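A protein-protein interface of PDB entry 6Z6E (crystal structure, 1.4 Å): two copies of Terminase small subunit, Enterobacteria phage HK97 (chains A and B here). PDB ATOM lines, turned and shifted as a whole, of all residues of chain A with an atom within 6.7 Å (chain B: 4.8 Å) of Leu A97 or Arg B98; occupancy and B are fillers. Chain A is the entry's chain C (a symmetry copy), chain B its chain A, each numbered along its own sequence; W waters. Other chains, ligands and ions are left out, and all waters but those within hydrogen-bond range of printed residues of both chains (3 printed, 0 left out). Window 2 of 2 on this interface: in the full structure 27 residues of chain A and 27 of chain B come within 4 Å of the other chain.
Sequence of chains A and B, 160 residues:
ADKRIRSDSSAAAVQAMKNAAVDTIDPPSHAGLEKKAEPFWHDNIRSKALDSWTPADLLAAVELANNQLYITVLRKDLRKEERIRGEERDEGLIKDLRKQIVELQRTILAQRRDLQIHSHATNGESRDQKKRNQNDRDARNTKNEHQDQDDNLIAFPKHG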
ATOM      1  N   TYR A  70       7.419  12.261  22.008  1.00  0.00           N
ATOM      2  CA  TYR A  70       7.111  11.568  20.764  1.00  0.00           C
ATOM      3  C   TYR A  70       6.387  12.414  19.755  1.00  0.00           C
ATOM      4  O   TYR A  70       6.592  12.248  18.561  1.00  0.00           O
ATOM      5  CB  TYR A  70       6.338  10.279  21.046  1.00  0.00           C
ATOM      6  CG  TYR A  70       6.393   9.228  19.952  1.00  0.00           C
ATOM      7  CD1 TYR A  70       7.597   8.859  19.350  1.00  0.00           C
ATOM      8  CD2 TYR A  70       5.283   8.529  19.596  1.00  0.00           C
ATOM      9  CE1 TYR A  70       7.648   7.869  18.402  1.00  0.00           C
ATOM     10  CE2 TYR A  70       5.321   7.506  18.660  1.00  0.00           C
ATOM     11  CZ  TYR A  70       6.511   7.181  18.070  1.00  0.00           C
ATOM     12  OH  TYR A  70       6.566   6.162  17.141  1.00  0.00           O
ATOM     13  N   VAL A  73       8.984  13.981  17.677  1.00  0.00           N
ATOM     14  CA  VAL A  73       9.583  12.997  16.784  1.00  0.00           C
ATOM     15  C   VAL A  73       8.698  12.772  15.571  1.00  0.00           C
ATOM     16  O   VAL A  73       9.150  12.818  14.415  1.00  0.00           O
ATOM     17  CB  VAL A  73       9.860  11.677  17.548  1.00  0.00           C
ATOM     18  CG1 VAL A  73      10.298  10.570  16.616  1.00  0.00           C
ATOM     19  CG2 VAL A  73      10.882  11.913  18.646  1.00  0.00           C
ATOM     20  N   LEU A  74       7.396  12.552  15.805  1.00  0.00           N
ATOM     21  CA  LEU A  74       6.488  12.352  14.691  1.00  0.00           C
ATOM     22  C   LEU A  74       6.339  13.596  13.826  1.00  0.00           C
ATOM     23  O   LEU A  74       6.219  13.474  12.617  1.00  0.00           O
ATOM     24  CB  LEU A  74       5.114  11.901  15.172  1.00  0.00           C
ATOM     25  CG  LEU A  74       5.116  10.571  15.906  1.00  0.00           C
ATOM     26  CD1 LEU A  74       3.682  10.168  16.147  1.00  0.00           C
ATOM     27  CD2 LEU A  74       5.851   9.487  15.097  1.00  0.00           C
ATOM     28  N   ARG A  75       6.352  14.781  14.429  1.00  0.00           N
ATOM     29  CA  ARG A  75       6.294  15.996  13.625  1.00  0.00           C
ATOM     30  C   ARG A  75       7.506  16.138  12.724  1.00  0.00           C
ATOM     31  O   ARG A  75       7.365  16.535  11.568  1.00  0.00           O
ATOM     32  CB  ARG A  75       6.121  17.237  14.514  1.00  0.00           C
ATOM     33  CG  ARG A  75       5.948  18.499  13.679  1.00  0.00           C
ATOM     34  CD  ARG A  75       5.532  19.713  14.458  1.00  0.00           C
ATOM     35  NE  ARG A  75       4.161  19.600  14.931  1.00  0.00           N
ATOM     36  CZ  ARG A  75       3.778  19.473  16.191  1.00  0.00           C
ATOM     37  NH1 ARG A  75       4.644  19.397  17.180  1.00  0.00           N
ATOM     38  NH2 ARG A  75       2.488  19.417  16.420  1.00  0.00           N
ATOM     39  N   ASP A  77       9.148  13.645  11.397  1.00  0.00           N
ATOM     40  CA  ASP A  77       8.914  12.711  10.310  1.00  0.00           C
ATOM     41  C   ASP A  77       7.891  13.267   9.330  1.00  0.00           C
ATOM     42  O   ASP A  77       8.032  13.142   8.124  1.00  0.00           O
ATOM     43  CB  ASP A  77       8.403  11.366  10.812  1.00  0.00           C
ATOM     44  CG  ASP A  77       9.456  10.524  11.505  1.00  0.00           C
ATOM     45  OD1 ASP A  77      10.670  10.822  11.422  1.00  0.00           O
ATOM     46  OD2 ASP A  77       9.034   9.543  12.179  1.00  0.00           O
ATOM     47  N   LEU A  78       6.839  13.881   9.856  1.00  0.00           N
ATOM     48  CA  LEU A  78       5.802  14.447   9.037  1.00  0.00           C
ATOM     49  C   LEU A  78       6.324  15.567   8.137  1.00  0.00           C
ATOM     50  O   LEU A  78       6.015  15.609   6.957  1.00  0.00           O
ATOM     51  CB  LEU A  78       4.647  14.945   9.921  1.00  0.00           C
ATOM     52  CG  LEU A  78       3.516  15.764   9.283  1.00  0.00           C
ATOM     53  CD1 LEU A  78       2.826  15.032   8.166  1.00  0.00           C
ATOM     54  CD2 LEU A  78       2.526  16.144  10.374  1.00  0.00           C
ATOM     55  N   ARG A  79       7.098  16.459   8.724  1.00  0.00           N
ATOM     56  CA  ARG A  79       7.628  17.603   7.971  1.00  0.00           C
ATOM     57  C   ARG A  79       8.570  17.091   6.891  1.00  0.00           C
ATOM     58  O   ARG A  79       8.556  17.622   5.810  1.00  0.00           O
ATOM     59  CB  ARG A  79       8.340  18.574   8.876  1.00  0.00           C
ATOM     60  CG  ARG A  79       7.453  19.339   9.839  1.00  0.00           C
ATOM     61  CD  ARG A  79       6.569  20.372   9.181  1.00  0.00           C
ATOM     62  NE  ARG A  79       5.656  20.929  10.184  1.00  0.00           N
ATOM     63  CZ  ARG A  79       4.448  20.433  10.490  1.00  0.00           C
ATOM     64  NH1 ARG A  79       3.924  19.432   9.820  1.00  0.00           N
ATOM     65  NH2 ARG A  79       3.760  20.993  11.469  1.00  0.00           N
ATOM     66  N   GLU A  81       8.293  14.191   5.281  1.00  0.00           N
ATOM     67  CA  GLU A  81       7.448  13.682   4.231  1.00  0.00           C
ATOM     68  C   GLU A  81       6.761  14.794   3.429  1.00  0.00           C
ATOM     69  O   GLU A  81       6.578  14.706   2.218  1.00  0.00           O
ATOM     70  CB  GLU A  81       6.388  12.728   4.794  1.00  0.00           C
ATOM     71  CG  GLU A  81       6.922  11.447   5.399  1.00  0.00           C
ATOM     72  CD  GLU A  81       7.724  10.587   4.423  1.00  0.00           C
ATOM     73  OE1 GLU A  81       7.392  10.564   3.231  1.00  0.00           O
ATOM     74  OE2 GLU A  81       8.672   9.905   4.877  1.00  0.00           O
ATOM     75  N   GLY A  92      -0.482   8.810   2.002  1.00  0.00           N
ATOM     76  CA  GLY A  92      -1.016   7.948   3.060  1.00  0.00           C
ATOM     77  C   GLY A  92      -0.256   8.081   4.358  1.00  0.00           C
ATOM     78  O   GLY A  92      -0.871   8.149   5.445  1.00  0.00           O
ATOM     79  N   LEU A  93       1.074   8.130   4.265  1.00  0.00           N
ATOM     80  CA  LEU A  93       1.906   8.272   5.439  1.00  0.00           C
ATOM     81  C   LEU A  93       1.685   9.646   6.090  1.00  0.00           C
ATOM     82  O   LEU A  93       1.613   9.758   7.333  1.00  0.00           O
ATOM     83  CB  LEU A  93       3.387   8.052   5.107  1.00  0.00           C
ATOM     84  CG  LEU A  93       4.358   8.155   6.265  1.00  0.00           C
ATOM     85  CD1 LEU A  93       4.003   7.275   7.464  1.00  0.00           C
ATOM     86  CD2 LEU A  93       5.762   7.818   5.738  1.00  0.00           C
ATOM     87  N   ILE A  94       1.593  10.673   5.261  1.00  0.00           N
ATOM     88  CA  ILE A  94       1.319  12.024   5.750  1.00  0.00           C
ATOM     89  C   ILE A  94      -0.004  12.035   6.536  1.00  0.00           C
ATOM     90  O   ILE A  94      -0.080  12.601   7.641  1.00  0.00           O
ATOM     91  CB  ILE A  94       1.312  13.044   4.591  1.00  0.00           C
ATOM     92  CG1 ILE A  94       2.749  13.256   4.082  1.00  0.00           C
ATOM     93  CG2 ILE A  94       0.712  14.373   5.030  1.00  0.00           C
ATOM     94  CD1 ILE A  94       2.840  13.979   2.744  1.00  0.00           C
ATOM     95  N   LYS A  95      -1.034  11.456   5.962  1.00  0.00           N
ATOM     96  CA  LYS A  95      -2.345  11.386   6.622  1.00  0.00           C
ATOM     97  C   LYS A  95      -2.255  10.649   7.948  1.00  0.00           C
ATOM     98  O   LYS A  95      -2.789  11.085   8.973  1.00  0.00           O
ATOM     99  CB  LYS A  95      -3.343  10.716   5.692  1.00  0.00           C
ATOM    100  CG  LYS A  95      -4.721  10.482   6.278  1.00  0.00           C
ATOM    101  CD  LYS A  95      -5.647   9.904   5.240  1.00  0.00           C
ATOM    102  CE  LYS A  95      -7.044   9.627   5.780  1.00  0.00           C
ATOM    103  NZ  LYS A  95      -7.919   9.096   4.696  1.00  0.00           N
ATOM    104  N   ASP A  96      -1.544   9.527   7.961  1.00  0.00           N
ATOM    105  CA  ASP A  96      -1.440   8.724   9.182  1.00  0.00           C
ATOM    106  C   ASP A  96      -0.686   9.452  10.290  1.00  0.00           C
ATOM    107  O   ASP A  96      -1.066   9.379  11.465  1.00  0.00           O
ATOM    108  CB  ASP A  96      -0.798   7.366   8.877  1.00  0.00           C
ATOM    109  CG  ASP A  96      -1.708   6.458   8.039  1.00  0.00           C
ATOM    110  OD1 ASP A  96      -2.910   6.696   7.976  1.00  0.00           O
ATOM    111  OD2 ASP A  96      -1.176   5.488   7.440  1.00  0.00           O
ATOM    112  N   LEU A  97       0.406  10.152   9.944  1.00  0.00           N
ATOM    113  CA  LEU A  97       1.178  10.918  10.917  1.00  0.00           C
ATOM    114  C   LEU A  97       0.359  12.076  11.497  1.00  0.00           C
ATOM    115  O   LEU A  97       0.430  12.341  12.686  1.00  0.00           O
ATOM    116  CB  LEU A  97       2.459  11.447  10.259  1.00  0.00           C
ATOM    117  CG  LEU A  97       3.535  10.379  10.076  1.00  0.00           C
ATOM    118  CD1 LEU A  97       4.589  10.879   9.087  1.00  0.00           C
ATOM    119  CD2 LEU A  97       4.209  10.028  11.374  1.00  0.00           C
ATOM    120  N   ARG A  98      -0.395  12.754  10.651  1.00  0.00           N
ATOM    121  CA  ARG A  98      -1.263  13.861  11.147  1.00  0.00           C
ATOM    122  C   ARG A  98      -2.203  13.340  12.212  1.00  0.00           C
ATOM    123  O   ARG A  98      -2.367  13.983  13.280  1.00  0.00           O
ATOM    124  CB  ARG A  98      -2.033  14.515  10.025  1.00  0.00           C
ATOM    125  CG  ARG A  98      -1.167  15.375   9.135  1.00  0.00           C
ATOM    126  CD  ARG A  98      -1.906  15.954   7.949  1.00  0.00           C
ATOM    127  NE  ARG A  98      -1.000  16.776   7.171  1.00  0.00           N
ATOM    128  CZ  ARG A  98      -1.164  17.099   5.892  1.00  0.00           C
ATOM    129  NH1 ARG A  98      -2.244  16.762   5.224  1.00  0.00           N
ATOM    130  NH2 ARG A  98      -0.191  17.780   5.271  1.00  0.00           N
ATOM    131  N   LYS A  99      -2.791  12.174  11.961  1.00  0.00           N
ATOM    132  CA  LYS A  99      -3.740  11.594  12.920  1.00  0.00           C
ATOM    133  C   LYS A  99      -3.039  11.117  14.171  1.00  0.00           C
ATOM    134  O   LYS A  99      -3.543  11.288  15.293  1.00  0.00           O
ATOM    135  CB  LYS A  99      -4.531  10.464  12.252  1.00  0.00           C
ATOM    136  CG  LYS A  99      -5.521   9.753  13.169  1.00  0.00           C
ATOM    137  CD  LYS A  99      -6.571  10.713  13.701  1.00  0.00           C
ATOM    138  CE  LYS A  99      -8.009  10.173  13.661  1.00  0.00           C
ATOM    139  NZ  LYS A  99      -8.969  11.255  13.273  1.00  0.00           N
ATOM    140  N   GLN A 100      -1.877  10.497  14.026  1.00  0.00           N
ATOM    141  CA  GLN A 100      -1.131  10.042  15.196  1.00  0.00           C
ATOM    142  C   GLN A 100      -0.784  11.182  16.148  1.00  0.00           C
ATOM    143  O   GLN A 100      -0.836  11.036  17.372  1.00  0.00           O
ATOM    144  CB  GLN A 100       0.108   9.264  14.798  1.00  0.00           C
ATOM    145  CG  GLN A 100      -0.242   7.898  14.204  1.00  0.00           C
ATOM    146  CD  GLN A 100       0.810   7.346  13.286  1.00  0.00           C
ATOM    147  OE1 GLN A 100       1.883   7.936  13.112  1.00  0.00           O
ATOM    148  NE2 GLN A 100       0.520   6.175  12.711  1.00  0.00           N
ATOM    149  N   ILE A 101      -0.411  12.335  15.576  1.00  0.00           N
ATOM    150  CA  ILE A 101      -0.121  13.495  16.401  1.00  0.00           C
ATOM    151  C   ILE A 101      -1.354  13.966  17.159  1.00  0.00           C
ATOM    152  O   ILE A 101      -1.271  14.218  18.371  1.00  0.00           O
ATOM    153  CB  ILE A 101       0.541  14.631  15.568  1.00  0.00           C
ATOM    154  CG1 ILE A 101       1.939  14.199  15.160  1.00  0.00           C
ATOM    155  CG2 ILE A 101       0.528  15.937  16.353  1.00  0.00           C
ATOM    156  CD1 ILE A 101       2.525  15.064  14.077  1.00  0.00           C
ATOM    157  N   VAL A 102      -2.481  14.067  16.488  1.00  0.00           N
ATOM    158  CA  VAL A 102      -3.734  14.474  17.142  1.00  0.00           C
ATOM    159  C   VAL A 102      -4.096  13.482  18.243  1.00  0.00           C
ATOM    160  O   VAL A 102      -4.502  13.886  19.346  1.00  0.00           O
ATOM    161  CB  VAL A 102      -4.870  14.633  16.107  1.00  0.00           C
ATOM    162  CG1 VAL A 102      -6.249  14.649  16.772  1.00  0.00           C
ATOM    163  CG2 VAL A 102      -4.639  15.892  15.290  1.00  0.00           C
ATOM    164  N   LEU A 104      -2.076  11.556  20.008  1.00  0.00           N
ATOM    165  CA  LEU A 104      -1.160  11.802  21.132  1.00  0.00           C
ATOM    166  C   LEU A 104      -1.560  13.035  21.904  1.00  0.00           C
ATOM    167  O   LEU A 104      -1.555  13.033  23.141  1.00  0.00           O
ATOM    168  CB  LEU A 104       0.293  11.953  20.661  1.00  0.00           C
ATOM    169  CG  LEU A 104       0.947  10.654  20.308  1.00  0.00           C
ATOM    170  CD1 LEU A 104       2.234  10.955  19.536  1.00  0.00           C
ATOM    171  CD2 LEU A 104       1.255   9.867  21.580  1.00  0.00           C
ATOM    172  N   LEU B  78       8.420  -1.138  18.729  1.00  0.00           N
ATOM    173  CA  LEU B  78       8.204  -0.013  17.847  1.00  0.00           C
ATOM    174  C   LEU B  78       9.498   0.653  17.433  1.00  0.00           C
ATOM    175  O   LEU B  78       9.681   0.945  16.268  1.00  0.00           O
ATOM    176  CB  LEU B  78       7.252   0.983  18.531  1.00  0.00           C
ATOM    177  CG  LEU B  78       6.980   2.319  17.857  1.00  0.00           C
ATOM    178  CD1 LEU B  78       6.425   2.169  16.447  1.00  0.00           C
ATOM    179  CD2 LEU B  78       6.009   3.129  18.718  1.00  0.00           C
ATOM    180  N   GLU B  82      11.032   1.156  13.738  1.00  0.00           N
ATOM    181  CA  GLU B  82      11.324   2.502  13.231  1.00  0.00           C
ATOM    182  C   GLU B  82      12.760   2.665  12.707  1.00  0.00           C
ATOM    183  O   GLU B  82      13.006   3.561  11.893  1.00  0.00           O
ATOM    184  CB  GLU B  82      11.061   3.548  14.310  1.00  0.00           C
ATOM    185  CG  GLU B  82       9.578   3.750  14.545  1.00  0.00           C
ATOM    186  CD  GLU B  82       9.301   4.655  15.735  1.00  0.00           C
ATOM    187  OE1 GLU B  82      10.018   4.602  16.744  1.00  0.00           O
ATOM    188  OE2 GLU B  82       8.363   5.431  15.635  1.00  0.00           O
ATOM    189  N   ILE B  94       4.182  -0.445  12.301  1.00  0.00           N
ATOM    190  CA  ILE B  94       4.499   0.778  13.042  1.00  0.00           C
ATOM    191  C   ILE B  94       3.209   1.513  13.435  1.00  0.00           C
ATOM    192  O   ILE B  94       3.069   1.932  14.592  1.00  0.00           O
ATOM    193  CB  ILE B  94       5.440   1.674  12.216  1.00  0.00           C
ATOM    194  CG1 ILE B  94       6.839   1.050  12.148  1.00  0.00           C
ATOM    195  CG2 ILE B  94       5.521   3.080  12.806  1.00  0.00           C
ATOM    196  CD1 ILE B  94       7.735   1.669  11.086  1.00  0.00           C
ATOM    197  N   LYS B  95       2.298   1.664  12.503  1.00  0.00           N
ATOM    198  CA  LYS B  95       1.005   2.304  12.769  1.00  0.00           C
ATOM    199  C   LYS B  95       0.237   1.563  13.853  1.00  0.00           C
ATOM    200  O   LYS B  95      -0.300   2.154  14.789  1.00  0.00           O
ATOM    201  CB  LYS B  95       0.189   2.397  11.492  1.00  0.00           C
ATOM    202  CG  LYS B  95      -1.218   2.938  11.636  1.00  0.00           C
ATOM    203  CD  LYS B  95      -1.840   3.198  10.278  1.00  0.00           C
ATOM    204  CE  LYS B  95      -3.236   3.787  10.402  1.00  0.00           C
ATOM    205  NZ  LYS B  95      -3.934   3.806   9.078  1.00  0.00           N
ATOM    206  N   ASP B  96       0.207   0.238  13.754  1.00  0.00           N
ATOM    207  CA  ASP B  96      -0.543  -0.562  14.732  1.00  0.00           C
ATOM    208  C   ASP B  96       0.053  -0.471  16.128  1.00  0.00           C
ATOM    209  O   ASP B  96      -0.696  -0.393  17.106  1.00  0.00           O
ATOM    210  CB  ASP B  96      -0.646  -2.024  14.263  1.00  0.00           C
ATOM    211  CG  ASP B  96      -1.544  -2.189  13.043  1.00  0.00           C
ATOM    212  OD1 ASP B  96      -2.334  -1.294  12.716  1.00  0.00           O
ATOM    213  OD2 ASP B  96      -1.413  -3.256  12.386  1.00  0.00           O
ATOM    214  N   LEU B  97       1.377  -0.506  16.250  1.00  0.00           N
ATOM    215  CA  LEU B  97       2.047  -0.396  17.538  1.00  0.00           C
ATOM    216  C   LEU B  97       1.822   0.981  18.169  1.00  0.00           C
ATOM    217  O   LEU B  97       1.590   1.077  19.379  1.00  0.00           O
ATOM    218  CB  LEU B  97       3.540  -0.650  17.382  1.00  0.00           C
ATOM    219  CG  LEU B  97       3.934  -2.107  17.189  1.00  0.00           C
ATOM    220  CD1 LEU B  97       5.352  -2.188  16.656  1.00  0.00           C
ATOM    221  CD2 LEU B  97       3.812  -2.856  18.501  1.00  0.00           C
ATOM    222  N   ARG B  98       1.856   2.026  17.366  1.00  0.00           N
ATOM    223  CA  ARG B  98       1.592   3.387  17.897  1.00  0.00           C
ATOM    224  C   ARG B  98       0.223   3.436  18.533  1.00  0.00           C
ATOM    225  O   ARG B  98       0.059   3.983  19.652  1.00  0.00           O
ATOM    226  CB  ARG B  98       1.709   4.454  16.814  1.00  0.00           C
ATOM    227  CG  ARG B  98       3.165   4.717  16.444  1.00  0.00           C
ATOM    228  CD  ARG B  98       3.302   5.679  15.283  1.00  0.00           C
ATOM    229  NE  ARG B  98       4.701   5.876  15.003  1.00  0.00           N
ATOM    230  CZ  ARG B  98       5.202   6.317  13.840  1.00  0.00           C
ATOM    231  NH1 ARG B  98       4.430   6.676  12.837  1.00  0.00           N
ATOM    232  NH2 ARG B  98       6.525   6.363  13.711  1.00  0.00           N
ATOM    233  N   LYS B  99      -0.764   2.859  17.850  1.00  0.00           N
ATOM    234  CA  LYS B  99      -2.133   2.861  18.359  1.00  0.00           C
ATOM    235  C   LYS B  99      -2.272   1.966  19.578  1.00  0.00           C
ATOM    236  O   LYS B  99      -2.965   2.324  20.550  1.00  0.00           O
ATOM    237  CB  LYS B  99      -3.108   2.442  17.259  1.00  0.00           C
ATOM    238  CG  LYS B  99      -4.579   2.402  17.703  1.00  0.00           C
ATOM    239  CD  LYS B  99      -5.523   1.899  16.620  1.00  0.00           C
ATOM    240  N   GLN B 100      -1.624   0.805  19.568  1.00  0.00           N
ATOM    241  CA  GLN B 100      -1.708  -0.079  20.729  1.00  0.00           C
ATOM    242  C   GLN B 100      -1.167   0.574  21.998  1.00  0.00           C
ATOM    243  O   GLN B 100      -1.708   0.386  23.089  1.00  0.00           O
ATOM    244  CB  GLN B 100      -0.978  -1.400  20.463  1.00  0.00           C
ATOM    245  CG  GLN B 100      -1.737  -2.289  19.498  1.00  0.00           C
ATOM    246  CD  GLN B 100      -0.883  -3.278  18.738  1.00  0.00           C
ATOM    247  OE1 GLN B 100       0.309  -3.402  18.960  1.00  0.00           O
ATOM    248  NE2 GLN B 100      -1.538  -4.026  17.850  1.00  0.00           N
ATOM    249  N   ILE B 101      -0.082   1.336  21.868  1.00  0.00           N
ATOM    250  CA  ILE B 101       0.483   2.037  23.007  1.00  0.00           C
ATOM    251  C   ILE B 101      -0.502   3.089  23.530  1.00  0.00           C
ATOM    252  O   ILE B 101      -0.733   3.151  24.750  1.00  0.00           O
ATOM    253  CB  ILE B 101       1.868   2.670  22.691  1.00  0.00           C
ATOM    254  CG1 ILE B 101       2.877   1.540  22.530  1.00  0.00           C
ATOM    255  CG2 ILE B 101       2.285   3.632  23.803  1.00  0.00           C
ATOM    256  CD1 ILE B 101       4.183   1.978  21.912  1.00  0.00           C
ATOM    257  N   VAL B 102      -1.102   3.868  22.640  1.00  0.00           N
ATOM    258  CA  VAL B 102      -2.083   4.873  23.058  1.00  0.00           C
ATOM    259  C   VAL B 102      -3.266   4.188  23.744  1.00  0.00           C
ATOM    260  O   VAL B 102      -3.762   4.671  24.775  1.00  0.00           O
ATOM    261  CB  VAL B 102      -2.524   5.739  21.867  1.00  0.00           C
ATOM    262  CG1 VAL B 102      -3.840   6.463  22.116  1.00  0.00           C
ATOM    263  CG2 VAL B 102      -1.383   6.700  21.493  1.00  0.00           C
HETATM  264  O   HOH W   1       7.298   7.733  11.348  1.00  0.00           O
HETATM  265  O   HOH W   2      -1.487   4.667  14.603  1.00  0.00           O
HETATM  266  O   HOH W   3       9.965   7.707  13.842  1.00  0.00           O
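OE2 of Glu B82 is in salt-bridge range of NH2 of Arg B98.
Of the 11 printed residues of chain B, 4 touch a printed residue of chain A. Hydrophobic or aromatic side chains of chain B within 4 Å of the printed part of chain A: Leu B78. Printed residues of chain A that touch a printed residue of chain B: Tyr A70, Leu A74, Asp A96, Leu A97 and Gln A100. Hydrophobic or aromatic side chains of chain A that line the printed part of chain B: Tyr A70, Leu A74 and Leu A97. Among the printed residues, 8 pairs touch across the chains.
Among the printed residues, pairs that only touch across the chains: Tyr A70 with Leu B78 (3.5 Å), Leu A74 with Arg B98 (3.5 Å), Leu A97 with Arg B98 (3.7 Å) and Gln A100 with Lys B95 (3.8 Å).
Water W1 bridges the side-chain carboxylate of Asp A77 (2.6 Å) and the guanidinium group of Arg B98 (2.8 Å). Water W3 bridges OD2 of Asp A77 (2.6 Å) and OE2 of Glu B82 (3.3 Å). Water W2 lies within hydrogen-bond range of the backbone carbonyl oxygen (O) of Lys B95 and the side-chain amide nitrogen (NE2) of Gln A100.
Of the printed residues of chain A, Arg B98 touches Tyr A70 (2.9 Å), Leu A74 (3.5 Å), Leu A97 (3.7 Å) and Gln A100 (2.9 Å). Of the printed residues of chain B, Asp A96 touches Lys B95 (3.3 Å). Of the printed residues of chain A, Leu B78 touches Tyr A70 (3.5 Å). Val A102 touches none of the printed residues of chain B. The nearest residue of chain A that does not touch Arg B98 is Asp A77 (4.3 Å). The nearest printed residue of chain B that does not touch Tyr A70 is Ile B94 (5.4 Å).
Asp A96 touches Lys B95, but with the chains exchanged Lys A95 does not touch Asp B96 (12.2 Å). Leu A97 touches Arg B98, but with the chains exchanged Arg A98 does not touch Leu B97 (14.1 Å). Gln A100 touches Lys B95, but with the chains exchanged Lys A95 does not touch Gln B100 (14.8 Å). Gln A100 touches Arg B98, but with the chains exchanged Arg A98 does not touch Gln B100 (14.5 Å). Of the 8 pairs that touch across the chains among the printed residues, none has its exchanged pair printed and touching as well.
OE2 of Glu B82 sits at hydrogen-bond distance from OH of Tyr A70, 2.5 Å away. The side-chain amino group (NZ) of Lys B95 is in salt-bridge range of the side-chain carboxylate (OD1) of Asp A96, at 3.3 Å. NE of Arg B98 sits at hydrogen-bond distance from OH of Tyr A70 (2.9 Å). OE1 of Gln A100 sits at hydrogen-bond distance from NH1 of Arg B98, 2.9 Å away.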
